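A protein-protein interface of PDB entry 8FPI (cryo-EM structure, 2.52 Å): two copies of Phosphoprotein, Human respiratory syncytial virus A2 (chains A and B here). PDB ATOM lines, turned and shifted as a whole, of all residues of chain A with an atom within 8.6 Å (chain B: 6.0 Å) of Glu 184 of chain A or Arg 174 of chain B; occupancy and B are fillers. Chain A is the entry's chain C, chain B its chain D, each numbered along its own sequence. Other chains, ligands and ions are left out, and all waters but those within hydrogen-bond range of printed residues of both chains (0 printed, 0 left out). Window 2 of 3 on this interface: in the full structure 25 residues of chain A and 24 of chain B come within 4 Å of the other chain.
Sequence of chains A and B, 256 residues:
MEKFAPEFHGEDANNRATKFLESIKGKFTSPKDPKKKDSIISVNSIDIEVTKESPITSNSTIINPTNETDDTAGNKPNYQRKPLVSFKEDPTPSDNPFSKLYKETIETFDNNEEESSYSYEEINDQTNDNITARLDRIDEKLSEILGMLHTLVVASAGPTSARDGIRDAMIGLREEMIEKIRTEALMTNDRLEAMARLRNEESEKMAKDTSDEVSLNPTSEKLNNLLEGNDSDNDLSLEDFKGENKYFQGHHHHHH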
ATOM      1  N   LEU A 173     -27.787 -16.310  10.850  1.00  0.00           N
ATOM      2  CA  LEU A 173     -26.656 -17.202  11.056  1.00  0.00           C
ATOM      3  C   LEU A 173     -25.808 -16.735  12.230  1.00  0.00           C
ATOM      4  O   LEU A 173     -25.719 -15.543  12.526  1.00  0.00           O
ATOM      5  CB  LEU A 173     -25.798 -17.273   9.801  1.00  0.00           C
ATOM      6  CG  LEU A 173     -26.401 -18.004   8.608  1.00  0.00           C
ATOM      7  CD1 LEU A 173     -27.438 -17.152   7.929  1.00  0.00           C
ATOM      8  CD2 LEU A 173     -25.314 -18.392   7.629  1.00  0.00           C
ATOM      9  N   MET A 177     -21.884 -21.703  12.812  1.00  0.00           N
ATOM     10  CA  MET A 177     -22.200 -21.978  11.421  1.00  0.00           C
ATOM     11  C   MET A 177     -21.362 -21.167  10.444  1.00  0.00           C
ATOM     12  O   MET A 177     -20.960 -21.693   9.399  1.00  0.00           O
ATOM     13  CB  MET A 177     -23.688 -21.709  11.157  1.00  0.00           C
ATOM     14  CG  MET A 177     -24.288 -22.621  10.106  1.00  0.00           C
ATOM     15  SD  MET A 177     -25.735 -21.910   9.305  1.00  0.00           S
ATOM     16  CE  MET A 177     -26.651 -23.395   8.897  1.00  0.00           C
ATOM     17  N   ILE A 178     -21.055 -19.919  10.765  1.00  0.00           N
ATOM     18  CA  ILE A 178     -20.140 -19.144   9.939  1.00  0.00           C
ATOM     19  C   ILE A 178     -18.740 -19.736   9.983  1.00  0.00           C
ATOM     20  O   ILE A 178     -18.041 -19.743   8.973  1.00  0.00           O
ATOM     21  CB  ILE A 178     -20.149 -17.671  10.385  1.00  0.00           C
ATOM     22  CG1 ILE A 178     -21.576 -17.115  10.304  1.00  0.00           C
ATOM     23  CG2 ILE A 178     -19.171 -16.863   9.543  1.00  0.00           C
ATOM     24  CD1 ILE A 178     -21.708 -15.758   9.678  1.00  0.00           C
ATOM     25  N   GLU A 179     -18.307 -20.228  11.143  1.00  0.00           N
ATOM     26  CA  GLU A 179     -17.026 -20.916  11.239  1.00  0.00           C
ATOM     27  C   GLU A 179     -16.962 -22.070  10.257  1.00  0.00           C
ATOM     28  O   GLU A 179     -15.970 -22.243   9.541  1.00  0.00           O
ATOM     29  CB  GLU A 179     -16.818 -21.432  12.659  1.00  0.00           C
ATOM     30  CG  GLU A 179     -16.058 -20.487  13.552  1.00  0.00           C
ATOM     31  CD  GLU A 179     -16.388 -20.682  15.014  1.00  0.00           C
ATOM     32  OE1 GLU A 179     -16.206 -19.729  15.796  1.00  0.00           O
ATOM     33  OE2 GLU A 179     -16.822 -21.792  15.383  1.00  0.00           O
ATOM     34  N   LYS A 180     -18.015 -22.883  10.221  1.00  0.00           N
ATOM     35  CA  LYS A 180     -18.075 -23.954   9.247  1.00  0.00           C
ATOM     36  C   LYS A 180     -18.034 -23.432   7.824  1.00  0.00           C
ATOM     37  O   LYS A 180     -17.358 -24.037   6.988  1.00  0.00           O
ATOM     38  CB  LYS A 180     -19.339 -24.783   9.440  1.00  0.00           C
ATOM     39  CG  LYS A 180     -19.743 -25.548   8.195  1.00  0.00           C
ATOM     40  CD  LYS A 180     -20.519 -26.802   8.513  1.00  0.00           C
ATOM     41  CE  LYS A 180     -20.776 -27.601   7.245  1.00  0.00           C
ATOM     42  NZ  LYS A 180     -22.166 -28.105   7.143  1.00  0.00           N
ATOM     43  N   ILE A 181     -18.739 -22.340   7.520  1.00  0.00           N
ATOM     44  CA  ILE A 181     -18.673 -21.817   6.157  1.00  0.00           C
ATOM     45  C   ILE A 181     -17.247 -21.393   5.806  1.00  0.00           C
ATOM     46  O   ILE A 181     -16.789 -21.622   4.683  1.00  0.00           O
ATOM     47  CB  ILE A 181     -19.672 -20.667   5.937  1.00  0.00           C
ATOM     48  CG1 ILE A 181     -21.097 -21.113   6.270  1.00  0.00           C
ATOM     49  CG2 ILE A 181     -19.636 -20.210   4.493  1.00  0.00           C
ATOM     50  CD1 ILE A 181     -21.938 -20.050   6.943  1.00  0.00           C
ATOM     51  N   ARG A 182     -16.518 -20.778   6.741  1.00  0.00           N
ATOM     52  CA  ARG A 182     -15.115 -20.469   6.460  1.00  0.00           C
ATOM     53  C   ARG A 182     -14.320 -21.737   6.188  1.00  0.00           C
ATOM     54  O   ARG A 182     -13.674 -21.864   5.144  1.00  0.00           O
ATOM     55  CB  ARG A 182     -14.426 -19.711   7.601  1.00  0.00           C
ATOM     56  CG  ARG A 182     -15.234 -18.843   8.507  1.00  0.00           C
ATOM     57  CD  ARG A 182     -15.027 -17.405   8.143  1.00  0.00           C
ATOM     58  NE  ARG A 182     -13.634 -17.007   8.290  1.00  0.00           N
ATOM     59  CZ  ARG A 182     -13.057 -16.701   9.442  1.00  0.00           C
ATOM     60  NH1 ARG A 182     -11.779 -16.363   9.467  1.00  0.00           N
ATOM     61  NH2 ARG A 182     -13.751 -16.721  10.569  1.00  0.00           N
ATOM     62  N   THR A 183     -14.371 -22.695   7.113  1.00  0.00           N
ATOM     63  CA  THR A 183     -13.564 -23.900   6.971  1.00  0.00           C
ATOM     64  C   THR A 183     -13.865 -24.543   5.628  1.00  0.00           C
ATOM     65  O   THR A 183     -12.994 -25.174   5.024  1.00  0.00           O
ATOM     66  CB  THR A 183     -13.825 -24.889   8.106  1.00  0.00           C
ATOM     67  OG1 THR A 183     -15.190 -25.316   8.064  1.00  0.00           O
ATOM     68  CG2 THR A 183     -13.519 -24.260   9.452  1.00  0.00           C
ATOM     69  N   GLU A 184     -15.098 -24.391   5.150  1.00  0.00           N
ATOM     70  CA  GLU A 184     -15.412 -24.820   3.795  1.00  0.00           C
ATOM     71  C   GLU A 184     -14.752 -23.918   2.761  1.00  0.00           C
ATOM     72  O   GLU A 184     -14.381 -24.384   1.678  1.00  0.00           O
ATOM     73  CB  GLU A 184     -16.925 -24.849   3.600  1.00  0.00           C
ATOM     74  CG  GLU A 184     -17.382 -25.754   2.480  1.00  0.00           C
ATOM     75  CD  GLU A 184     -18.841 -25.567   2.148  1.00  0.00           C
ATOM     76  OE1 GLU A 184     -19.219 -25.775   0.976  1.00  0.00           O
ATOM     77  OE2 GLU A 184     -19.614 -25.218   3.064  1.00  0.00           O
ATOM     78  N   ALA A 185     -14.603 -22.630   3.069  1.00  0.00           N
ATOM     79  CA  ALA A 185     -13.955 -21.694   2.156  1.00  0.00           C
ATOM     80  C   ALA A 185     -12.471 -21.971   1.980  1.00  0.00           C
ATOM     81  O   ALA A 185     -11.865 -21.421   1.055  1.00  0.00           O
ATOM     82  CB  ALA A 185     -14.142 -20.261   2.653  1.00  0.00           C
ATOM     83  N   LEU A 186     -11.879 -22.799   2.832  1.00  0.00           N
ATOM     84  CA  LEU A 186     -10.453 -23.093   2.777  1.00  0.00           C
ATOM     85  C   LEU A 186     -10.199 -24.494   2.233  1.00  0.00           C
ATOM     86  O   LEU A 186     -10.579 -24.813   1.109  1.00  0.00           O
ATOM     87  CB  LEU A 186      -9.839 -22.952   4.168  1.00  0.00           C
ATOM     88  CG  LEU A 186      -8.323 -23.118   4.260  1.00  0.00           C
ATOM     89  CD1 LEU A 186      -7.615 -21.915   3.663  1.00  0.00           C
ATOM     90  CD2 LEU A 186      -7.907 -23.331   5.706  1.00  0.00           C
ATOM     91  N   ALA B 169     -32.718 -18.730  -1.628  1.00  0.00           N
ATOM     92  CA  ALA B 169     -31.954 -17.514  -1.407  1.00  0.00           C
ATOM     93  C   ALA B 169     -31.021 -17.622  -0.209  1.00  0.00           C
ATOM     94  O   ALA B 169     -30.124 -16.786  -0.063  1.00  0.00           O
ATOM     95  CB  ALA B 169     -32.904 -16.336  -1.239  1.00  0.00           C
ATOM     96  N   MET B 170     -31.215 -18.616   0.655  1.00  0.00           N
ATOM     97  CA  MET B 170     -30.250 -18.919   1.704  1.00  0.00           C
ATOM     98  C   MET B 170     -29.146 -19.849   1.221  1.00  0.00           C
ATOM     99  O   MET B 170     -28.005 -19.731   1.682  1.00  0.00           O
ATOM    100  CB  MET B 170     -30.958 -19.540   2.912  1.00  0.00           C
ATOM    101  CG  MET B 170     -31.725 -18.554   3.767  1.00  0.00           C
ATOM    102  SD  MET B 170     -30.760 -17.120   4.247  1.00  0.00           S
ATOM    103  CE  MET B 170     -30.068 -17.716   5.781  1.00  0.00           C
ATOM    104  N   ILE B 171     -29.453 -20.759   0.297  1.00  0.00           N
ATOM    105  CA  ILE B 171     -28.395 -21.435  -0.438  1.00  0.00           C
ATOM    106  C   ILE B 171     -27.497 -20.399  -1.092  1.00  0.00           C
ATOM    107  O   ILE B 171     -26.265 -20.492  -1.039  1.00  0.00           O
ATOM    108  CB  ILE B 171     -28.991 -22.391  -1.485  1.00  0.00           C
ATOM    109  CG1 ILE B 171     -29.513 -23.664  -0.824  1.00  0.00           C
ATOM    110  CG2 ILE B 171     -27.948 -22.743  -2.537  1.00  0.00           C
ATOM    111  CD1 ILE B 171     -30.646 -24.317  -1.597  1.00  0.00           C
ATOM    112  N   GLY B 172     -28.105 -19.397  -1.721  1.00  0.00           N
ATOM    113  CA  GLY B 172     -27.329 -18.311  -2.277  1.00  0.00           C
ATOM    114  C   GLY B 172     -26.509 -17.584  -1.233  1.00  0.00           C
ATOM    115  O   GLY B 172     -25.341 -17.269  -1.466  1.00  0.00           O
ATOM    116  N   LEU B 173     -27.100 -17.306  -0.068  1.00  0.00           N
ATOM    117  CA  LEU B 173     -26.345 -16.644   0.991  1.00  0.00           C
ATOM    118  C   LEU B 173     -25.092 -17.427   1.343  1.00  0.00           C
ATOM    119  O   LEU B 173     -23.990 -16.868   1.368  1.00  0.00           O
ATOM    120  CB  LEU B 173     -27.203 -16.475   2.242  1.00  0.00           C
ATOM    121  CG  LEU B 173     -26.927 -15.190   3.025  1.00  0.00           C
ATOM    122  CD1 LEU B 173     -27.534 -13.993   2.318  1.00  0.00           C
ATOM    123  CD2 LEU B 173     -27.421 -15.301   4.457  1.00  0.00           C
ATOM    124  N   ARG B 174     -25.239 -18.721   1.628  1.00  0.00           N
ATOM    125  CA  ARG B 174     -24.077 -19.501   2.033  1.00  0.00           C
ATOM    126  C   ARG B 174     -23.058 -19.596   0.906  1.00  0.00           C
ATOM    127  O   ARG B 174     -21.858 -19.419   1.138  1.00  0.00           O
ATOM    128  CB  ARG B 174     -24.494 -20.899   2.483  1.00  0.00           C
ATOM    129  CG  ARG B 174     -23.313 -21.846   2.632  1.00  0.00           C
ATOM    130  CD  ARG B 174     -23.627 -23.013   3.536  1.00  0.00           C
ATOM    131  NE  ARG B 174     -22.621 -24.065   3.431  1.00  0.00           N
ATOM    132  CZ  ARG B 174     -22.688 -25.228   4.070  1.00  0.00           C
ATOM    133  NH1 ARG B 174     -21.728 -26.128   3.912  1.00  0.00           N
ATOM    134  NH2 ARG B 174     -23.718 -25.502   4.860  1.00  0.00           N
ATOM    135  N   GLU B 175     -23.505 -19.857  -0.319  1.00  0.00           N
ATOM    136  CA  GLU B 175     -22.569 -20.095  -1.410  1.00  0.00           C
ATOM    137  C   GLU B 175     -21.960 -18.813  -1.960  1.00  0.00           C
ATOM    138  O   GLU B 175     -21.031 -18.893  -2.769  1.00  0.00           O
ATOM    139  CB  GLU B 175     -23.260 -20.872  -2.534  1.00  0.00           C
ATOM    140  CG  GLU B 175     -23.702 -20.036  -3.721  1.00  0.00           C
ATOM    141  CD  GLU B 175     -24.503 -20.843  -4.716  1.00  0.00           C
ATOM    142  OE1 GLU B 175     -24.826 -20.306  -5.795  1.00  0.00           O
ATOM    143  OE2 GLU B 175     -24.806 -22.018  -4.423  1.00  0.00           O
ATOM    144  N   GLU B 176     -22.461 -17.645  -1.559  1.00  0.00           N
ATOM    145  CA  GLU B 176     -21.829 -16.383  -1.908  1.00  0.00           C
ATOM    146  C   GLU B 176     -21.051 -15.792  -0.743  1.00  0.00           C
ATOM    147  O   GLU B 176     -20.212 -14.913  -0.962  1.00  0.00           O
ATOM    148  CB  GLU B 176     -22.884 -15.380  -2.406  1.00  0.00           C
ATOM    149  CG  GLU B 176     -22.650 -13.928  -2.024  1.00  0.00           C
ATOM    150  CD  GLU B 176     -23.780 -13.030  -2.476  1.00  0.00           C
ATOM    151  OE1 GLU B 176     -24.492 -13.408  -3.430  1.00  0.00           O
ATOM    152  OE2 GLU B 176     -23.958 -11.949  -1.876  1.00  0.00           O
ATOM    153  N   MET B 177     -21.307 -16.242   0.483  1.00  0.00           N
ATOM    154  CA  MET B 177     -20.461 -15.902   1.617  1.00  0.00           C
ATOM    155  C   MET B 177     -19.108 -16.585   1.533  1.00  0.00           C
ATOM    156  O   MET B 177     -18.092 -15.989   1.905  1.00  0.00           O
ATOM    157  CB  MET B 177     -21.145 -16.311   2.918  1.00  0.00           C
ATOM    158  CG  MET B 177     -21.222 -15.223   3.950  1.00  0.00           C
ATOM    159  SD  MET B 177     -21.949 -15.860   5.458  1.00  0.00           S
ATOM    160  CE  MET B 177     -23.357 -14.774   5.574  1.00  0.00           C
ATOM    161  N   ILE B 178     -19.083 -17.830   1.054  1.00  0.00           N
ATOM    162  CA  ILE B 178     -17.833 -18.533   0.804  1.00  0.00           C
ATOM    163  C   ILE B 178     -17.037 -17.891  -0.319  1.00  0.00           C
ATOM    164  O   ILE B 178     -15.799 -17.948  -0.299  1.00  0.00           O
ATOM    165  CB  ILE B 178     -18.120 -20.011   0.470  1.00  0.00           C
ATOM    166  CG1 ILE B 178     -16.842 -20.847   0.543  1.00  0.00           C
ATOM    167  CG2 ILE B 178     -18.750 -20.133  -0.908  1.00  0.00           C
ATOM    168  CD1 ILE B 178     -16.979 -22.229  -0.067  1.00  0.00           C
ATOM    169  N   GLU B 179     -17.704 -17.271  -1.291  1.00  0.00           N
ATOM    170  CA  GLU B 179     -17.029 -16.647  -2.419  1.00  0.00           C
ATOM    171  C   GLU B 179     -16.413 -15.302  -2.074  1.00  0.00           C
ATOM    172  O   GLU B 179     -15.409 -14.927  -2.687  1.00  0.00           O
ATOM    173  CB  GLU B 179     -18.005 -16.463  -3.586  1.00  0.00           C
ATOM    174  CG  GLU B 179     -18.708 -17.739  -4.015  1.00  0.00           C
ATOM    175  CD  GLU B 179     -18.033 -18.411  -5.189  1.00  0.00           C
ATOM    176  OE1 GLU B 179     -16.810 -18.646  -5.117  1.00  0.00           O
ATOM    177  OE2 GLU B 179     -18.725 -18.703  -6.185  1.00  0.00           O
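Of chain B, only Arg 174 (2.5 Å) and Ile 178 (3.8 Å) come within 4 Å of Glu 184 of chain A. Of the printed residues of chain A, Arg 174 of chain B touches Lys 180 and Glu 184. No residue of chain A comes within 4 Å of Gly 172 of chain B. Of the printed residues of chain B, Lys 180 of chain A touches Arg 174. Of the printed residues of chain A, Met 170 of chain B touches Leu 173 (3.4 Å). Of the printed residues of chain A, Ile 178 of chain B touches Glu 184 (3.8 Å) and Ala 185 (3.4 Å). Printed residues of chain B within 4 Å of Leu 173 of chain A: Met 170 and Leu 173. Met 177 of chain A touches none of the printed residues of chain B. The nearest residue of chain A that does not touch Arg 174 of chain B is Ile 181 of chain A (4.1 Å).
The side-chain carboxylate (OE2) of Glu 184 of chain A lies within salt-bridge range of the guanidinium group (NH1) of Arg 174 of chain B.
Printed residues of chain B that touch a printed residue of chain A: Met 170, Leu 173, Arg 174 and Ile 178. Hydrophobic or aromatic side chains of chain B that line the printed part of chain A: Met 170, Leu 173 and Ile 178. Hydrophobic or aromatic side chains of chain A within 4 Å of the printed part of chain B: Leu 173 and Ala 185. Among the printed residues, 6 pairs touch across the chains.
Among the printed residues, pairs that only touch across the chains: Leu 173 of chain A with Met 170 of chain B (3.4 Å), Leu 173 of chain A with Leu 173 of chain B (3.9 Å), Lys 180 of chain A with Arg 174 of chain B (3.8 Å), Glu 184 of chain A with Ile 178 of chain B (3.8 Å) and Ala 185 of chain A with Ile 178 of chain B (3.4 Å).
O of Lys 180 of chain A is in hydrogen-bond range of OG1 of Thr 183 of chain A, 2.7 Å away.
Leu 173 of chain A touches its own counterpart, Leu 173 of chain B.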
